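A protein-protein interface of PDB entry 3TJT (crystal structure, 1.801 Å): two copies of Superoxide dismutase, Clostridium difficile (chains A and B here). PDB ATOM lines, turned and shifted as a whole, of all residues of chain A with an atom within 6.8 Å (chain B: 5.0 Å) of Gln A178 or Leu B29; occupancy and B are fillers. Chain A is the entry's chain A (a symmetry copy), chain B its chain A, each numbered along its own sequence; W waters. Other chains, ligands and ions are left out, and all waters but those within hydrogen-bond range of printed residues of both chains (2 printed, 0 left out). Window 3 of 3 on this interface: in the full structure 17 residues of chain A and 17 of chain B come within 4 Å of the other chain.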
ATOM      1  N   GLU A 170      -3.449 -22.215  -9.092  1.00  0.00           N
ATOM      2  CA  GLU A 170      -2.248 -21.392  -9.096  1.00  0.00           C
ATOM      3  C   GLU A 170      -2.245 -20.327 -10.199  1.00  0.00           C
ATOM      4  O   GLU A 170      -1.634 -19.270 -10.021  1.00  0.00           O
ATOM      5  CB  GLU A 170      -0.992 -22.278  -9.111  1.00  0.00           C
ATOM      6  CG  GLU A 170      -0.774 -22.943  -7.754  1.00  0.00           C
ATOM      7  CD  GLU A 170       0.297 -24.029  -7.761  1.00  0.00           C
ATOM      8  OE1 GLU A 170       0.470 -24.712  -8.797  1.00  0.00           O
ATOM      9  OE2 GLU A 170       0.954 -24.185  -6.716  1.00  0.00           O
ATOM     10  N   TYR A 173      -3.047 -16.689  -9.034  1.00  0.00           N
ATOM     11  CA  TYR A 173      -2.227 -15.897  -8.133  1.00  0.00           C
ATOM     12  C   TYR A 173      -0.711 -16.003  -8.313  1.00  0.00           C
ATOM     13  O   TYR A 173       0.023 -15.269  -7.657  1.00  0.00           O
ATOM     14  CB  TYR A 173      -2.576 -16.188  -6.666  1.00  0.00           C
ATOM     15  CG  TYR A 173      -2.291 -17.603  -6.167  1.00  0.00           C
ATOM     16  CD1 TYR A 173      -1.025 -17.965  -5.698  1.00  0.00           C
ATOM     17  CD2 TYR A 173      -3.302 -18.559  -6.124  1.00  0.00           C
ATOM     18  CE1 TYR A 173      -0.777 -19.268  -5.203  1.00  0.00           C
ATOM     19  CE2 TYR A 173      -3.061 -19.858  -5.640  1.00  0.00           C
ATOM     20  CZ  TYR A 173      -1.806 -20.201  -5.185  1.00  0.00           C
ATOM     21  OH  TYR A 173      -1.582 -21.481  -4.705  1.00  0.00           O
ATOM     22  N   TYR A 174      -0.239 -16.893  -9.180  1.00  0.00           N
ATOM     23  CA  TYR A 174       1.199 -17.173  -9.203  1.00  0.00           C
ATOM     24  C   TYR A 174       2.064 -16.002  -9.706  1.00  0.00           C
ATOM     25  O   TYR A 174       3.163 -15.777  -9.196  1.00  0.00           O
ATOM     26  CB  TYR A 174       1.527 -18.481  -9.952  1.00  0.00           C
ATOM     27  CG  TYR A 174       2.690 -19.190  -9.292  1.00  0.00           C
ATOM     28  CD1 TYR A 174       2.515 -19.876  -8.098  1.00  0.00           C
ATOM     29  CD2 TYR A 174       3.967 -19.128  -9.835  1.00  0.00           C
ATOM     30  CE1 TYR A 174       3.581 -20.507  -7.463  1.00  0.00           C
ATOM     31  CE2 TYR A 174       5.051 -19.757  -9.202  1.00  0.00           C
ATOM     32  CZ  TYR A 174       4.846 -20.434  -8.021  1.00  0.00           C
ATOM     33  OH  TYR A 174       5.899 -21.051  -7.389  1.00  0.00           O
ATOM     34  N   LEU A 175       1.577 -15.244 -10.680  1.00  0.00           N
ATOM     35  CA  LEU A 175       2.410 -14.159 -11.216  1.00  0.00           C
ATOM     36  C   LEU A 175       2.739 -13.097 -10.176  1.00  0.00           C
ATOM     37  O   LEU A 175       3.853 -12.569 -10.152  1.00  0.00           O
ATOM     38  CB  LEU A 175       1.769 -13.511 -12.444  1.00  0.00           C
ATOM     39  CG  LEU A 175       1.650 -14.384 -13.690  1.00  0.00           C
ATOM     40  CD1 LEU A 175       1.069 -13.569 -14.839  1.00  0.00           C
ATOM     41  CD2 LEU A 175       3.001 -14.989 -14.075  1.00  0.00           C
ATOM     42  N   LYS A 176       1.772 -12.769  -9.324  1.00  0.00           N
ATOM     43  CA  LYS A 176       1.992 -11.745  -8.307  1.00  0.00           C
ATOM     44  C   LYS A 176       2.460 -12.293  -6.963  1.00  0.00           C
ATOM     45  O   LYS A 176       3.328 -11.700  -6.314  1.00  0.00           O
ATOM     46  CB  LYS A 176       0.732 -10.905  -8.121  1.00  0.00           C
ATOM     47  CG  LYS A 176       0.859  -9.840  -7.048  1.00  0.00           C
ATOM     48  CD  LYS A 176      -0.384  -8.958  -7.029  1.00  0.00           C
ATOM     49  CE  LYS A 176      -0.227  -7.826  -6.027  1.00  0.00           C
ATOM     50  NZ  LYS A 176       0.584  -6.704  -6.569  1.00  0.00           N
ATOM     51  N   TYR A 177       1.902 -13.430  -6.546  1.00  0.00           N
ATOM     52  CA  TYR A 177       2.131 -13.937  -5.201  1.00  0.00           C
ATOM     53  C   TYR A 177       3.005 -15.197  -5.139  1.00  0.00           C
ATOM     54  O   TYR A 177       3.409 -15.607  -4.061  1.00  0.00           O
ATOM     55  CB  TYR A 177       0.787 -14.235  -4.523  1.00  0.00           C
ATOM     56  CG  TYR A 177      -0.053 -12.994  -4.355  1.00  0.00           C
ATOM     57  CD1 TYR A 177       0.190 -12.115  -3.310  1.00  0.00           C
ATOM     58  CD2 TYR A 177      -1.057 -12.690  -5.255  1.00  0.00           C
ATOM     59  CE1 TYR A 177      -0.559 -10.961  -3.153  1.00  0.00           C
ATOM     60  CE2 TYR A 177      -1.824 -11.525  -5.106  1.00  0.00           C
ATOM     61  CZ  TYR A 177      -1.567 -10.676  -4.055  1.00  0.00           C
ATOM     62  OH  TYR A 177      -2.320  -9.528  -3.900  1.00  0.00           O
ATOM     63  N   GLN A 178       3.274 -15.790  -6.295  1.00  0.00           N
ATOM     64  CA  GLN A 178       3.998 -17.061  -6.386  1.00  0.00           C
ATOM     65  C   GLN A 178       3.391 -18.053  -5.398  1.00  0.00           C
ATOM     66  O   GLN A 178       2.172 -18.234  -5.409  1.00  0.00           O
ATOM     67  CB  GLN A 178       5.504 -16.858  -6.189  1.00  0.00           C
ATOM     68  CG  GLN A 178       6.133 -16.005  -7.301  1.00  0.00           C
ATOM     69  CD  GLN A 178       5.977 -14.504  -7.061  1.00  0.00           C
ATOM     70  OE1 GLN A 178       6.371 -13.990  -6.018  1.00  0.00           O
ATOM     71  NE2 GLN A 178       5.402 -13.799  -8.033  1.00  0.00           N
ATOM     72  N   ASN A 179       4.206 -18.668  -4.542  1.00  0.00           N
ATOM     73  CA  ASN A 179       3.706 -19.680  -3.598  1.00  0.00           C
ATOM     74  C   ASN A 179       2.921 -19.127  -2.413  1.00  0.00           C
ATOM     75  O   ASN A 179       2.362 -19.892  -1.612  1.00  0.00           O
ATOM     76  CB  ASN A 179       4.869 -20.494  -3.037  1.00  0.00           C
ATOM     77  CG  ASN A 179       5.840 -19.634  -2.264  1.00  0.00           C
ATOM     78  OD1 ASN A 179       6.482 -18.748  -2.833  1.00  0.00           O
ATOM     79  ND2 ASN A 179       5.932 -19.866  -0.964  1.00  0.00           N
ATOM     80  N   ARG A 180       2.914 -17.806  -2.267  1.00  0.00           N
ATOM     81  CA  ARG A 180       2.343 -17.177  -1.078  1.00  0.00           C
ATOM     82  C   ARG A 180       0.826 -17.026  -1.203  1.00  0.00           C
ATOM     83  O   ARG A 180       0.291 -15.912  -1.225  1.00  0.00           O
ATOM     84  CB  ARG A 180       3.032 -15.824  -0.809  1.00  0.00           C
ATOM     85  CG  ARG A 180       4.570 -15.956  -0.711  1.00  0.00           C
ATOM     86  CD  ARG A 180       5.262 -14.607  -0.465  1.00  0.00           C
ATOM     87  NE  ARG A 180       4.933 -13.626  -1.499  1.00  0.00           N
ATOM     88  CZ  ARG A 180       5.475 -13.604  -2.709  1.00  0.00           C
ATOM     89  NH1 ARG A 180       6.374 -14.517  -3.052  1.00  0.00           N
ATOM     90  NH2 ARG A 180       5.111 -12.677  -3.587  1.00  0.00           N
ATOM     91  N   ARG A 181       0.128 -18.158  -1.266  1.00  0.00           N
ATOM     92  CA  ARG A 181      -1.321 -18.122  -1.443  1.00  0.00           C
ATOM     93  C   ARG A 181      -2.005 -17.349  -0.310  1.00  0.00           C
ATOM     94  O   ARG A 181      -3.015 -16.669  -0.524  1.00  0.00           O
ATOM     95  CB  ARG A 181      -1.903 -19.538  -1.566  1.00  0.00           C
ATOM     96  CG  ARG A 181      -3.378 -19.533  -1.990  1.00  0.00           C
ATOM     97  CD  ARG A 181      -4.072 -20.869  -1.667  1.00  0.00           C
ATOM     98  NE  ARG A 181      -3.576 -21.956  -2.501  1.00  0.00           N
ATOM     99  CZ  ARG A 181      -3.982 -23.220  -2.387  1.00  0.00           C
ATOM    100  NH1 ARG A 181      -4.905 -23.545  -1.486  1.00  0.00           N
ATOM    101  NH2 ARG A 181      -3.472 -24.157  -3.177  1.00  0.00           N
ATOM    102  N   GLU B  25      14.123 -18.442 -11.643  1.00  0.00           N
ATOM    103  CA  GLU B  25      13.225 -18.010 -10.579  1.00  0.00           C
ATOM    104  C   GLU B  25      12.297 -19.159 -10.173  1.00  0.00           C
ATOM    105  O   GLU B  25      12.040 -19.383  -8.987  1.00  0.00           O
ATOM    106  CB  GLU B  25      12.421 -16.794 -11.036  1.00  0.00           C
ATOM    107  CG  GLU B  25      13.275 -15.536 -11.261  1.00  0.00           C
ATOM    108  CD  GLU B  25      14.240 -15.611 -12.457  1.00  0.00           C
ATOM    109  OE1 GLU B  25      13.945 -16.304 -13.463  1.00  0.00           O
ATOM    110  OE2 GLU B  25      15.301 -14.938 -12.388  1.00  0.00           O
ATOM    111  N   THR B  26      11.816 -19.884 -11.169  1.00  0.00           N
ATOM    112  CA  THR B  26      10.953 -21.040 -10.916  1.00  0.00           C
ATOM    113  C   THR B  26      11.707 -22.177 -10.228  1.00  0.00           C
ATOM    114  O   THR B  26      11.188 -22.809  -9.307  1.00  0.00           O
ATOM    115  CB  THR B  26      10.302 -21.516 -12.214  1.00  0.00           C
ATOM    116  OG1 THR B  26       9.361 -20.533 -12.647  1.00  0.00           O
ATOM    117  CG2 THR B  26       9.580 -22.853 -12.014  1.00  0.00           C
ATOM    118  N   MET B  27      12.942 -22.435 -10.647  1.00  0.00           N
ATOM    119  CA  MET B  27      13.726 -23.461  -9.956  1.00  0.00           C
ATOM    120  C   MET B  27      13.894 -23.133  -8.475  1.00  0.00           C
ATOM    121  O   MET B  27      13.778 -24.011  -7.622  1.00  0.00           O
ATOM    122  CB  MET B  27      15.099 -23.670 -10.624  1.00  0.00           C
ATOM    123  CG  MET B  27      15.026 -24.167 -12.067  1.00  0.00           C
ATOM    124  SD  MET B  27      14.177 -25.774 -12.292  1.00  0.00           S
ATOM    125  CE  MET B  27      15.092 -26.813 -11.159  1.00  0.00           C
ATOM    126  N   LYS B  28      14.157 -21.864  -8.166  1.00  0.00           N
ATOM    127  CA  LYS B  28      14.289 -21.424  -6.781  1.00  0.00           C
ATOM    128  C   LYS B  28      12.997 -21.635  -5.985  1.00  0.00           C
ATOM    129  O   LYS B  28      13.018 -22.197  -4.898  1.00  0.00           O
ATOM    130  CB  LYS B  28      14.710 -19.951  -6.715  1.00  0.00           C
ATOM    131  CG  LYS B  28      16.147 -19.692  -7.145  1.00  0.00           C
ATOM    132  CD  LYS B  28      17.068 -19.495  -5.942  1.00  0.00           C
ATOM    133  CE  LYS B  28      18.519 -19.275  -6.383  1.00  0.00           C
ATOM    134  NZ  LYS B  28      19.480 -19.317  -5.239  1.00  0.00           N
ATOM    135  N   LEU B  29      11.875 -21.186  -6.535  1.00  0.00           N
ATOM    136  CA  LEU B  29      10.603 -21.328  -5.837  1.00  0.00           C
ATOM    137  C   LEU B  29      10.235 -22.796  -5.720  1.00  0.00           C
ATOM    138  O   LEU B  29       9.833 -23.262  -4.659  1.00  0.00           O
ATOM    139  CB  LEU B  29       9.496 -20.597  -6.598  1.00  0.00           C
ATOM    140  CG  LEU B  29       9.532 -19.067  -6.541  1.00  0.00           C
ATOM    141  CD1 LEU B  29       8.713 -18.488  -7.677  1.00  0.00           C
ATOM    142  CD2 LEU B  29       9.044 -18.554  -5.205  1.00  0.00           C
ATOM    143  N   HIS B  30      10.364 -23.515  -6.821  1.00  0.00           N
ATOM    144  CA  HIS B  30       9.912 -24.904  -6.884  1.00  0.00           C
ATOM    145  C   HIS B  30      10.680 -25.746  -5.863  1.00  0.00           C
ATOM    146  O   HIS B  30      10.095 -26.543  -5.125  1.00  0.00           O
ATOM    147  CB  HIS B  30      10.120 -25.437  -8.300  1.00  0.00           C
ATOM    148  CG  HIS B  30       9.218 -26.578  -8.657  1.00  0.00           C
ATOM    149  ND1 HIS B  30       9.283 -27.211  -9.879  1.00  0.00           N
ATOM    150  CD2 HIS B  30       8.217 -27.181  -7.971  1.00  0.00           C
ATOM    151  CE1 HIS B  30       8.370 -28.166  -9.927  1.00  0.00           C
ATOM    152  NE2 HIS B  30       7.713 -28.169  -8.782  1.00  0.00           N
ATOM    153  N   HIS B  31      11.997 -25.564  -5.807  1.00  0.00           N
ATOM    154  CA  HIS B  31      12.817 -26.345  -4.883  1.00  0.00           C
ATOM    155  C   HIS B  31      12.807 -25.790  -3.458  1.00  0.00           C
ATOM    156  O   HIS B  31      12.567 -26.524  -2.495  1.00  0.00           O
ATOM    157  CB  HIS B  31      14.267 -26.429  -5.403  1.00  0.00           C
ATOM    158  CG  HIS B  31      15.183 -27.212  -4.515  1.00  0.00           C
ATOM    159  ND1 HIS B  31      15.739 -26.690  -3.367  1.00  0.00           N
ATOM    160  CD2 HIS B  31      15.644 -28.481  -4.614  1.00  0.00           C
ATOM    161  CE1 HIS B  31      16.497 -27.606  -2.791  1.00  0.00           C
ATOM    162  NE2 HIS B  31      16.460 -28.700  -3.531  1.00  0.00           N
ATOM    163  N   ASP B  32      13.067 -24.493  -3.315  1.00  0.00           N
ATOM    164  CA  ASP B  32      13.274 -23.908  -1.988  1.00  0.00           C
ATOM    165  C   ASP B  32      11.985 -23.620  -1.219  1.00  0.00           C
ATOM    166  O   ASP B  32      12.004 -23.548   0.004  1.00  0.00           O
ATOM    167  CB  ASP B  32      14.095 -22.617  -2.074  1.00  0.00           C
ATOM    168  CG  ASP B  32      15.481 -22.831  -2.660  1.00  0.00           C
ATOM    169  OD1 ASP B  32      15.874 -23.985  -2.916  1.00  0.00           O
ATOM    170  OD2 ASP B  32      16.183 -21.826  -2.878  1.00  0.00           O
ATOM    171  N   LYS B  33      10.879 -23.426  -1.934  1.00  0.00           N
ATOM    172  CA  LYS B  33       9.593 -23.191  -1.278  1.00  0.00           C
ATOM    173  C   LYS B  33       8.645 -24.399  -1.336  1.00  0.00           C
ATOM    174  O   LYS B  33       8.229 -24.907  -0.298  1.00  0.00           O
ATOM    175  CB  LYS B  33       8.892 -21.962  -1.863  1.00  0.00           C
ATOM    176  CG  LYS B  33       9.726 -20.698  -1.824  1.00  0.00           C
ATOM    177  CD  LYS B  33      10.052 -20.273  -0.412  1.00  0.00           C
ATOM    178  CE  LYS B  33      10.862 -18.976  -0.455  1.00  0.00           C
ATOM    179  NZ  LYS B  33      11.381 -18.606   0.883  1.00  0.00           N
ATOM    180  N   HIS B  34       8.293 -24.843  -2.540  1.00  0.00           N
ATOM    181  CA  HIS B  34       7.291 -25.910  -2.672  1.00  0.00           C
ATOM    182  C   HIS B  34       7.800 -27.256  -2.148  1.00  0.00           C
ATOM    183  O   HIS B  34       7.174 -27.876  -1.297  1.00  0.00           O
ATOM    184  CB  HIS B  34       6.818 -26.061  -4.120  1.00  0.00           C
ATOM    185  CG  HIS B  34       6.076 -24.871  -4.648  1.00  0.00           C
ATOM    186  ND1 HIS B  34       4.723 -24.688  -4.443  1.00  0.00           N
ATOM    187  CD2 HIS B  34       6.490 -23.809  -5.380  1.00  0.00           C
ATOM    188  CE1 HIS B  34       4.339 -23.565  -5.023  1.00  0.00           C
ATOM    189  NE2 HIS B  34       5.390 -23.011  -5.599  1.00  0.00           N
ATOM    190  N   TYR B  35       8.934 -27.709  -2.664  1.00  0.00           N
ATOM    191  CA  TYR B  35       9.497 -28.988  -2.225  1.00  0.00           C
ATOM    192  C   TYR B  35       9.770 -28.937  -0.717  1.00  0.00           C
ATOM    193  O   TYR B  35       9.363 -29.830   0.043  1.00  0.00           O
ATOM    194  CB  TYR B  35      10.736 -29.296  -3.081  1.00  0.00           C
ATOM    195  CG  TYR B  35      11.555 -30.517  -2.717  1.00  0.00           C
ATOM    196  CD1 TYR B  35      11.004 -31.608  -2.032  1.00  0.00           C
ATOM    197  CD2 TYR B  35      12.887 -30.595  -3.103  1.00  0.00           C
ATOM    198  CE1 TYR B  35      11.789 -32.729  -1.714  1.00  0.00           C
ATOM    199  CE2 TYR B  35      13.667 -31.697  -2.787  1.00  0.00           C
ATOM    200  CZ  TYR B  35      13.124 -32.755  -2.101  1.00  0.00           C
ATOM    201  OH  TYR B  35      13.944 -33.836  -1.822  1.00  0.00           O
ATOM    202  N   LEU B 175       5.324 -18.973 -14.432  1.00  0.00           N
ATOM    203  CA  LEU B 175       6.124 -17.748 -14.563  1.00  0.00           C
ATOM    204  C   LEU B 175       6.683 -17.553 -15.964  1.00  0.00           C
ATOM    205  O   LEU B 175       6.738 -16.428 -16.465  1.00  0.00           O
ATOM    206  CB  LEU B 175       7.256 -17.702 -13.534  1.00  0.00           C
ATOM    207  CG  LEU B 175       6.841 -17.584 -12.071  1.00  0.00           C
ATOM    208  CD1 LEU B 175       8.079 -17.468 -11.190  1.00  0.00           C
ATOM    209  CD2 LEU B 175       5.901 -16.397 -11.853  1.00  0.00           C
HETATM  210  O   HOH W   1       2.002 -25.953  -4.065  1.00  0.00           O
HETATM  211  O   HOH W   2       7.619 -22.884  -8.687  1.00  0.00           O
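Hydrophobic or aromatic side chains of chain B that line the printed part of chain A: Leu B29, His B34 and Leu B175. Of the 10 printed residues of chain A, 5 touch a printed residue of chain B. Hydrophobic or aromatic side chains of chain A that line the printed part of chain B: Tyr A174 and Leu A175. Among the printed residues, 9 pairs touch across the chains.
Of chain B, only Leu B29 (3.6 Å) comes within 4 Å of Gln A178. Leu B29 touches just these residues of chain A: Tyr A174 (3.7 Å), Gln A178 (3.6 Å) and Asn A179 (3.5 Å). Of the printed residues of chain A, His B34 touches Glu A170, Tyr A174 and Asn A179. Of the printed residues of chain B, Tyr A174 touches Leu B29, His B34 and Leu B175. Of the printed residues of chain B, Leu A175 touches Leu B175. Of the printed residues of chain B, Glu A170 touches His B34. Printed residues of chain A within 4 Å of Leu B175: Tyr A174 and Leu A175. The nearest residue of chain B that does not touch Gln A178 is Leu B175 (4.6 Å).
The backbone carbonyl oxygen of Leu B29 is in hydrogen-bond range of the backbone NH of His B34, 3.1 Å away. The backbone carbonyl oxygen (O) of Tyr A174 lies close to the side-chain amide nitrogen (NE2) of Gln A178 (3.2 Å). O of Leu A175 lies within hydrogen-bond range of NE2 of Gln A178 (2.9 Å). The side-chain amide nitrogen (NE2) of Gln A178 is in hydrogen-bond range of the backbone carbonyl oxygen (O) of Lys A176 (3.4 Å). The side-chain amide oxygen (OE1) of Gln A178 lies within hydrogen-bond range of the guanidinium group (NH1) of Arg A180 (3.0 Å).
Water W2 lies within hydrogen-bond range of the side-chain hydroxyl of Tyr A174 (2.8 Å) and the backbone NH of His B30 (3.4 Å). Water W1 bridges a ring nitrogen (ND1) of His B34 (3.0 Å) and the side-chain carboxylate (OE2) of Glu A170 (3.4 Å).
Leu A175 touches its own counterpart, Leu B175. 1 position is printed for both chains.
A ring nitrogen (NE2) of His B34 lies within hydrogen-bond range of the side-chain hydroxyl (OH) of Tyr A174 (2.7 Å).
Among the printed residues, merely in contact across the chains: Glu A170 with His B34, Tyr A174 with Leu B29, Tyr A174 with Leu B175, Leu A175 with Leu B175, Gln A178 with Leu B29, Asn A179 with Leu B29, Asn A179 with Lys B33 and Asn A179 with His B34.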
